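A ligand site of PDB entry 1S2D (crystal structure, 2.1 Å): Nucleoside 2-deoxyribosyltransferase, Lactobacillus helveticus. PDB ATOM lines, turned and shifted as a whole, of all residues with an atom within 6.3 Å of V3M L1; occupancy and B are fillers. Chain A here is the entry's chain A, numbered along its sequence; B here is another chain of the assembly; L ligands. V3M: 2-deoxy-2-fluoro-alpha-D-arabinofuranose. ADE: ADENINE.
C1 of V3M L1 is bonded to OE2 of Glu 101 (1.4 Å). The side-chain carboxylate (OD1) of Asp 95 is in hydrogen-bond range of an oxygen (O5) of V3M L1, 2.7 Å away. The side-chain amide oxygen of Asn 128 of chain B is in hydrogen-bond range of an oxygen (O5) of V3M L1, 2.9 Å away. The backbone NH (N) of Ser 14 sits at hydrogen-bond distance from an oxygen (O3) of V3M L1 (2.9 Å). An oxygen (O5) of V3M L1 sits at hydrogen-bond distance from the side-chain hydroxyl (OH) of Tyr 17. The backbone carbonyl oxygen (O) of Pro 44 lies within hydrogen-bond range of a nitrogen (N6) of ADE L2 (3.2 Å). The side-chain carboxylate (OD2) of Asp 75 lies within hydrogen-bond range of a nitrogen (N1) of ADE L2 (2.7 Å). OXT of Tyr 167 of chain B is in hydrogen-bond range of N9 of ADE L2 (2.8 Å).
The side-chain carboxylate (OE2) of Glu 101 lies within hydrogen-bond range of the side-chain hydroxyl (OH) of Tyr 11. The side-chain carboxylate (OD2) of Asp 95 sits close to the side-chain amide oxygen (OD1) of Asn 128 of chain B, 3.2 Å away. The side-chain carboxylate of Asp 95 is in hydrogen-bond range of the backbone NH of Gly 97 (3.1 Å). The side-chain hydroxyl of Ser 98 lies within hydrogen-bond range of the side-chain carboxylate of Asp 95. The backbone NH (N) of Met 130 of chain B sits close to the side-chain amide nitrogen (ND2) of Asn 128 of chain B, 3.0 Å away.
A fluorine (F2) of V3M L1 lies close to the side-chain carboxylate (OD2) of Asp 75, 3.3 Å away. The backbone carbonyl oxygen of Gly 97 lies close to an oxygen (O4) of V3M L1. Merely in contact with V3M L1: Tyr 11, Gly 13, Pro 44, Phe 45, Ser 98 and Met 130 of chain B. Hydrophobic or aromatic side chains within 4 Å of V3M L1: Tyr 17, Pro 44, Phe 45 and Met 130 of chain B. Within 4 Å of V3M L1: Tyr 11, Gly 13, Ser 14, Tyr 17, Pro 44, Phe 45, Asp 75, Asp 95, Gly 97, Ser 98, Glu 101, Asn 128 of chain B and Met 130 of chain B.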
ATOM      1  N   TYR A  11      11.829  10.192  22.815  1.00  0.00           N
ATOM      2  CA  TYR A  11      12.865   9.313  22.311  1.00  0.00           C
ATOM      3  C   TYR A  11      13.252   8.613  23.603  1.00  0.00           C
ATOM      4  O   TYR A  11      13.854   9.218  24.492  1.00  0.00           O
ATOM      5  CB  TYR A  11      14.078  10.084  21.761  1.00  0.00           C
ATOM      6  CG  TYR A  11      15.206   9.164  21.314  1.00  0.00           C
ATOM      7  CD1 TYR A  11      15.128   8.482  20.102  1.00  0.00           C
ATOM      8  CD2 TYR A  11      16.353   9.021  22.082  1.00  0.00           C
ATOM      9  CE1 TYR A  11      16.184   7.663  19.672  1.00  0.00           C
ATOM     10  CE2 TYR A  11      17.403   8.206  21.660  1.00  0.00           C
ATOM     11  CZ  TYR A  11      17.322   7.536  20.453  1.00  0.00           C
ATOM     12  OH  TYR A  11      18.388   6.797  20.010  1.00  0.00           O
ATOM     13  N   LEU A  12      12.807   7.374  23.746  1.00  0.00           N
ATOM     14  CA  LEU A  12      13.084   6.594  24.937  1.00  0.00           C
ATOM     15  C   LEU A  12      14.413   5.864  24.759  1.00  0.00           C
ATOM     16  O   LEU A  12      14.462   4.784  24.192  1.00  0.00           O
ATOM     17  CB  LEU A  12      11.932   5.619  25.185  1.00  0.00           C
ATOM     18  CG  LEU A  12      11.940   4.781  26.464  1.00  0.00           C
ATOM     19  CD1 LEU A  12      12.136   5.665  27.699  1.00  0.00           C
ATOM     20  CD2 LEU A  12      10.614   4.019  26.533  1.00  0.00           C
ATOM     21  N   GLY A  13      15.493   6.512  25.202  1.00  0.00           N
ATOM     22  CA  GLY A  13      16.808   5.917  25.090  1.00  0.00           C
ATOM     23  C   GLY A  13      17.088   4.965  26.223  1.00  0.00           C
ATOM     24  O   GLY A  13      16.780   5.257  27.377  1.00  0.00           O
ATOM     25  N   SER A  14      17.686   3.820  25.897  1.00  0.00           N
ATOM     26  CA  SER A  14      17.988   2.829  26.912  1.00  0.00           C
ATOM     27  C   SER A  14      18.794   1.623  26.443  1.00  0.00           C
ATOM     28  O   SER A  14      18.717   1.218  25.286  1.00  0.00           O
ATOM     29  CB  SER A  14      16.691   2.299  27.530  1.00  0.00           C
ATOM     30  OG  SER A  14      16.922   1.193  28.382  1.00  0.00           O
ATOM     31  N   PRO A  15      19.592   1.053  27.358  1.00  0.00           N
ATOM     32  CA  PRO A  15      20.401  -0.133  27.051  1.00  0.00           C
ATOM     33  C   PRO A  15      19.326  -1.233  26.990  1.00  0.00           C
ATOM     34  O   PRO A  15      18.221  -1.037  27.482  1.00  0.00           O
ATOM     35  CB  PRO A  15      21.259  -0.308  28.299  1.00  0.00           C
ATOM     36  CG  PRO A  15      21.332   1.057  28.883  1.00  0.00           C
ATOM     37  CD  PRO A  15      19.932   1.569  28.692  1.00  0.00           C
ATOM     38  N   PHE A  16      19.641  -2.387  26.422  1.00  0.00           N
ATOM     39  CA  PHE A  16      18.663  -3.461  26.321  1.00  0.00           C
ATOM     40  C   PHE A  16      19.478  -4.742  26.316  1.00  0.00           C
ATOM     41  O   PHE A  16      19.156  -5.717  25.631  1.00  0.00           O
ATOM     42  CB  PHE A  16      17.896  -3.296  25.002  1.00  0.00           C
ATOM     43  CG  PHE A  16      16.546  -3.937  24.995  1.00  0.00           C
ATOM     44  CD1 PHE A  16      15.513  -3.420  25.781  1.00  0.00           C
ATOM     45  CD2 PHE A  16      16.282  -5.047  24.198  1.00  0.00           C
ATOM     46  CE1 PHE A  16      14.255  -3.986  25.763  1.00  0.00           C
ATOM     47  CE2 PHE A  16      15.020  -5.624  24.168  1.00  0.00           C
ATOM     48  CZ  PHE A  16      14.000  -5.090  24.957  1.00  0.00           C
ATOM     49  N   TYR A  17      20.522  -4.724  27.145  1.00  0.00           N
ATOM     50  CA  TYR A  17      21.483  -5.812  27.219  1.00  0.00           C
ATOM     51  C   TYR A  17      21.370  -6.768  28.405  1.00  0.00           C
ATOM     52  O   TYR A  17      22.072  -7.778  28.458  1.00  0.00           O
ATOM     53  CB  TYR A  17      22.882  -5.190  27.096  1.00  0.00           C
ATOM     54  CG  TYR A  17      22.939  -4.113  26.003  1.00  0.00           C
ATOM     55  CD1 TYR A  17      22.526  -4.399  24.695  1.00  0.00           C
ATOM     56  CD2 TYR A  17      23.330  -2.799  26.283  1.00  0.00           C
ATOM     57  CE1 TYR A  17      22.497  -3.414  23.710  1.00  0.00           C
ATOM     58  CE2 TYR A  17      23.309  -1.788  25.279  1.00  0.00           C
ATOM     59  CZ  TYR A  17      22.883  -2.116  24.007  1.00  0.00           C
ATOM     60  OH  TYR A  17      22.863  -1.171  22.992  1.00  0.00           O
ATOM     61  N   PHE A  43      10.935   3.949  20.685  1.00  0.00           N
ATOM     62  CA  PHE A  43      11.882   3.072  21.351  1.00  0.00           C
ATOM     63  C   PHE A  43      12.675   2.362  20.264  1.00  0.00           C
ATOM     64  O   PHE A  43      12.148   1.518  19.537  1.00  0.00           O
ATOM     65  CB  PHE A  43      11.174   2.045  22.235  1.00  0.00           C
ATOM     66  CG  PHE A  43      12.107   1.270  23.137  1.00  0.00           C
ATOM     67  CD1 PHE A  43      12.938   1.942  24.027  1.00  0.00           C
ATOM     68  CD2 PHE A  43      12.174  -0.115  23.078  1.00  0.00           C
ATOM     69  CE1 PHE A  43      13.813   1.246  24.856  1.00  0.00           C
ATOM     70  CE2 PHE A  43      13.042  -0.832  23.897  1.00  0.00           C
ATOM     71  CZ  PHE A  43      13.870  -0.148  24.792  1.00  0.00           C
ATOM     72  N   PRO A  44      13.967   2.698  20.138  1.00  0.00           N
ATOM     73  CA  PRO A  44      14.884   2.137  19.145  1.00  0.00           C
ATOM     74  C   PRO A  44      14.936   0.619  18.979  1.00  0.00           C
ATOM     75  O   PRO A  44      15.132   0.134  17.858  1.00  0.00           O
ATOM     76  CB  PRO A  44      16.233   2.723  19.541  1.00  0.00           C
ATOM     77  CG  PRO A  44      16.075   3.068  20.999  1.00  0.00           C
ATOM     78  CD  PRO A  44      14.686   3.620  21.038  1.00  0.00           C
ATOM     79  N   PHE A  45      14.732  -0.126  20.058  1.00  0.00           N
ATOM     80  CA  PHE A  45      14.769  -1.580  19.977  1.00  0.00           C
ATOM     81  C   PHE A  45      13.490  -2.264  19.462  1.00  0.00           C
ATOM     82  O   PHE A  45      13.478  -3.469  19.264  1.00  0.00           O
ATOM     83  CB  PHE A  45      15.247  -2.185  21.303  1.00  0.00           C
ATOM     84  CG  PHE A  45      16.674  -1.837  21.639  1.00  0.00           C
ATOM     85  CD1 PHE A  45      16.960  -0.757  22.482  1.00  0.00           C
ATOM     86  CD2 PHE A  45      17.725  -2.550  21.085  1.00  0.00           C
ATOM     87  CE1 PHE A  45      18.277  -0.399  22.746  1.00  0.00           C
ATOM     88  CE2 PHE A  45      19.048  -2.195  21.341  1.00  0.00           C
ATOM     89  CZ  PHE A  45      19.326  -1.113  22.178  1.00  0.00           C
ATOM     90  N   ASP A  75      18.112   5.239  14.652  1.00  0.00           N
ATOM     91  CA  ASP A  75      18.313   5.809  15.981  1.00  0.00           C
ATOM     92  C   ASP A  75      18.385   7.339  15.912  1.00  0.00           C
ATOM     93  O   ASP A  75      17.784   8.015  16.746  1.00  0.00           O
ATOM     94  CB  ASP A  75      19.576   5.226  16.647  1.00  0.00           C
ATOM     95  CG  ASP A  75      19.424   3.750  16.986  1.00  0.00           C
ATOM     96  OD1 ASP A  75      18.284   3.227  16.994  1.00  0.00           O
ATOM     97  OD2 ASP A  75      20.449   3.082  17.245  1.00  0.00           O
ATOM     98  N   PHE A  87      15.900   9.100  29.117  1.00  0.00           N
ATOM     99  CA  PHE A  87      16.904   8.053  29.196  1.00  0.00           C
ATOM    100  C   PHE A  87      16.948   7.212  30.465  1.00  0.00           C
ATOM    101  O   PHE A  87      17.252   7.704  31.554  1.00  0.00           O
ATOM    102  CB  PHE A  87      18.295   8.661  28.932  1.00  0.00           C
ATOM    103  CG  PHE A  87      18.516   9.069  27.504  1.00  0.00           C
ATOM    104  CD1 PHE A  87      19.108   8.181  26.605  1.00  0.00           C
ATOM    105  CD2 PHE A  87      18.079  10.313  27.040  1.00  0.00           C
ATOM    106  CE1 PHE A  87      19.244   8.524  25.259  1.00  0.00           C
ATOM    107  CE2 PHE A  87      18.211  10.669  25.700  1.00  0.00           C
ATOM    108  CZ  PHE A  87      18.800   9.772  24.802  1.00  0.00           C
ATOM    109  N   ASP A  95      26.229   2.954  29.624  1.00  0.00           N
ATOM    110  CA  ASP A  95      25.928   2.680  28.226  1.00  0.00           C
ATOM    111  C   ASP A  95      26.394   3.853  27.374  1.00  0.00           C
ATOM    112  O   ASP A  95      25.797   4.932  27.409  1.00  0.00           O
ATOM    113  CB  ASP A  95      24.429   2.444  28.029  1.00  0.00           C
ATOM    114  CG  ASP A  95      24.046   2.218  26.579  1.00  0.00           C
ATOM    115  OD1 ASP A  95      22.879   2.498  26.221  1.00  0.00           O
ATOM    116  OD2 ASP A  95      24.906   1.765  25.782  1.00  0.00           O
ATOM    117  N   ASP A  96      27.468   3.649  26.620  1.00  0.00           N
ATOM    118  CA  ASP A  96      27.970   4.727  25.772  1.00  0.00           C
ATOM    119  C   ASP A  96      27.028   5.098  24.628  1.00  0.00           C
ATOM    120  O   ASP A  96      27.063   6.220  24.140  1.00  0.00           O
ATOM    121  CB  ASP A  96      29.395   4.438  25.264  1.00  0.00           C
ATOM    122  CG  ASP A  96      29.528   3.074  24.578  1.00  0.00           C
ATOM    123  OD1 ASP A  96      28.564   2.292  24.579  1.00  0.00           O
ATOM    124  OD2 ASP A  96      30.618   2.809  24.034  1.00  0.00           O
ATOM    125  N   GLY A  97      26.155   4.164  24.259  1.00  0.00           N
ATOM    126  CA  GLY A  97      25.187   4.422  23.213  1.00  0.00           C
ATOM    127  C   GLY A  97      24.238   5.503  23.685  1.00  0.00           C
ATOM    128  O   GLY A  97      23.970   6.462  22.953  1.00  0.00           O
ATOM    129  N   SER A  98      23.725   5.339  24.901  1.00  0.00           N
ATOM    130  CA  SER A  98      22.813   6.316  25.509  1.00  0.00           C
ATOM    131  C   SER A  98      23.547   7.639  25.732  1.00  0.00           C
ATOM    132  O   SER A  98      22.970   8.706  25.509  1.00  0.00           O
ATOM    133  CB  SER A  98      22.276   5.810  26.848  1.00  0.00           C
ATOM    134  OG  SER A  98      21.360   4.747  26.683  1.00  0.00           O
ATOM    135  N   ALA A  99      24.806   7.569  26.171  1.00  0.00           N
ATOM    136  CA  ALA A  99      25.561   8.796  26.429  1.00  0.00           C
ATOM    137  C   ALA A  99      25.770   9.595  25.133  1.00  0.00           C
ATOM    138  O   ALA A  99      25.604  10.817  25.126  1.00  0.00           O
ATOM    139  CB  ALA A  99      26.901   8.475  27.082  1.00  0.00           C
ATOM    140  N   GLU A 101      23.896   9.514  22.517  1.00  0.00           N
ATOM    141  CA  GLU A 101      22.582  10.027  22.190  1.00  0.00           C
ATOM    142  C   GLU A 101      22.186  11.255  23.019  1.00  0.00           C
ATOM    143  O   GLU A 101      21.583  12.197  22.481  1.00  0.00           O
ATOM    144  CB  GLU A 101      21.551   8.911  22.287  1.00  0.00           C
ATOM    145  CG  GLU A 101      21.841   7.786  21.263  1.00  0.00           C
ATOM    146  CD  GLU A 101      21.158   6.467  21.545  1.00  0.00           C
ATOM    147  OE1 GLU A 101      20.520   6.360  22.626  1.00  0.00           O
ATOM    148  OE2 GLU A 101      21.254   5.611  20.607  1.00  0.00           O
ATOM    149  N   ASN B 128      29.496  -0.437  20.742  1.00  0.00           N
ATOM    150  CA  ASN B 128      28.122   0.035  20.664  1.00  0.00           C
ATOM    151  C   ASN B 128      27.953   0.636  19.271  1.00  0.00           C
ATOM    152  O   ASN B 128      28.842   1.317  18.775  1.00  0.00           O
ATOM    153  CB  ASN B 128      27.861   1.107  21.737  1.00  0.00           C
ATOM    154  CG  ASN B 128      26.383   1.468  21.857  1.00  0.00           C
ATOM    155  OD1 ASN B 128      25.693   1.004  22.763  1.00  0.00           O
ATOM    156  ND2 ASN B 128      25.913   2.321  20.957  1.00  0.00           N
ATOM    157  N   MET B 130      26.295   3.152  18.140  1.00  0.00           N
ATOM    158  CA  MET B 130      26.399   4.619  18.072  1.00  0.00           C
ATOM    159  C   MET B 130      27.843   5.083  17.920  1.00  0.00           C
ATOM    160  O   MET B 130      28.122   6.055  17.209  1.00  0.00           O
ATOM    161  CB  MET B 130      25.755   5.274  19.287  1.00  0.00           C
ATOM    162  CG  MET B 130      24.285   4.912  19.481  1.00  0.00           C
ATOM    163  SD  MET B 130      23.296   4.958  17.955  1.00  0.00           S
ATOM    164  CE  MET B 130      23.080   6.712  17.742  1.00  0.00           C
ATOM    165  N   TYR B 167      26.391  -4.595  19.025  1.00  0.00           N
ATOM    166  CA  TYR B 167      25.232  -4.938  19.846  1.00  0.00           C
ATOM    167  C   TYR B 167      24.217  -3.801  19.940  1.00  0.00           C
ATOM    168  O   TYR B 167      24.622  -2.621  19.816  1.00  0.00           O
ATOM    169  CB  TYR B 167      25.678  -5.370  21.247  1.00  0.00           C
ATOM    170  CG  TYR B 167      26.555  -4.381  21.973  1.00  0.00           C
ATOM    171  CD1 TYR B 167      26.001  -3.444  22.855  1.00  0.00           C
ATOM    172  CD2 TYR B 167      27.938  -4.389  21.817  1.00  0.00           C
ATOM    173  CE1 TYR B 167      26.811  -2.546  23.551  1.00  0.00           C
ATOM    174  CE2 TYR B 167      28.758  -3.504  22.515  1.00  0.00           C
ATOM    175  CZ  TYR B 167      28.179  -2.574  23.378  1.00  0.00           C
ATOM    176  OH  TYR B 167      28.978  -1.687  24.055  1.00  0.00           O
ATOM    177  OXT TYR B 167      23.024  -4.112  20.140  1.00  0.00           O
HETATM  178  O5  V3M L   1      23.010   1.748  23.581  1.00  0.00           O
HETATM  179  C5  V3M L   1      21.677   1.779  23.040  1.00  0.00           C
HETATM  180  C4  V3M L   1      21.137   3.198  23.051  1.00  0.00           C
HETATM  181  O4  V3M L   1      21.809   4.135  22.192  1.00  0.00           O
HETATM  182  C1  V3M L   1      21.131   4.273  20.936  1.00  0.00           C
HETATM  183  C2  V3M L   1      19.674   3.945  21.224  1.00  0.00           C
HETATM  184  F2  V3M L   1      19.201   3.026  20.297  1.00  0.00           F
HETATM  185  C3  V3M L   1      19.723   3.316  22.609  1.00  0.00           C
HETATM  186  O3  V3M L   1      19.165   4.137  23.374  1.00  0.00           O
HETATM  187  N9  ADE L   2      21.112  -3.388  18.172  1.00  0.00           N
HETATM  188  C8  ADE L   2      19.986  -3.791  17.535  1.00  0.00           C
HETATM  189  N7  ADE L   2      19.126  -2.837  17.258  1.00  0.00           N
HETATM  190  C5  ADE L   2      19.774  -1.689  17.768  1.00  0.00           C
HETATM  191  C6  ADE L   2      19.401  -0.305  17.815  1.00  0.00           C
HETATM  192  N6  ADE L   2      18.254   0.141  17.299  1.00  0.00           N
HETATM  193  N1  ADE L   2      20.276   0.594  18.398  1.00  0.00           N
HETATM  194  C2  ADE L   2      21.454   0.150  18.926  1.00  0.00           C
HETATM  195  N3  ADE L   2      21.889  -1.136  18.930  1.00  0.00           N
HETATM  196  C4  ADE L   2      21.000  -2.011  18.337  1.00  0.00           C
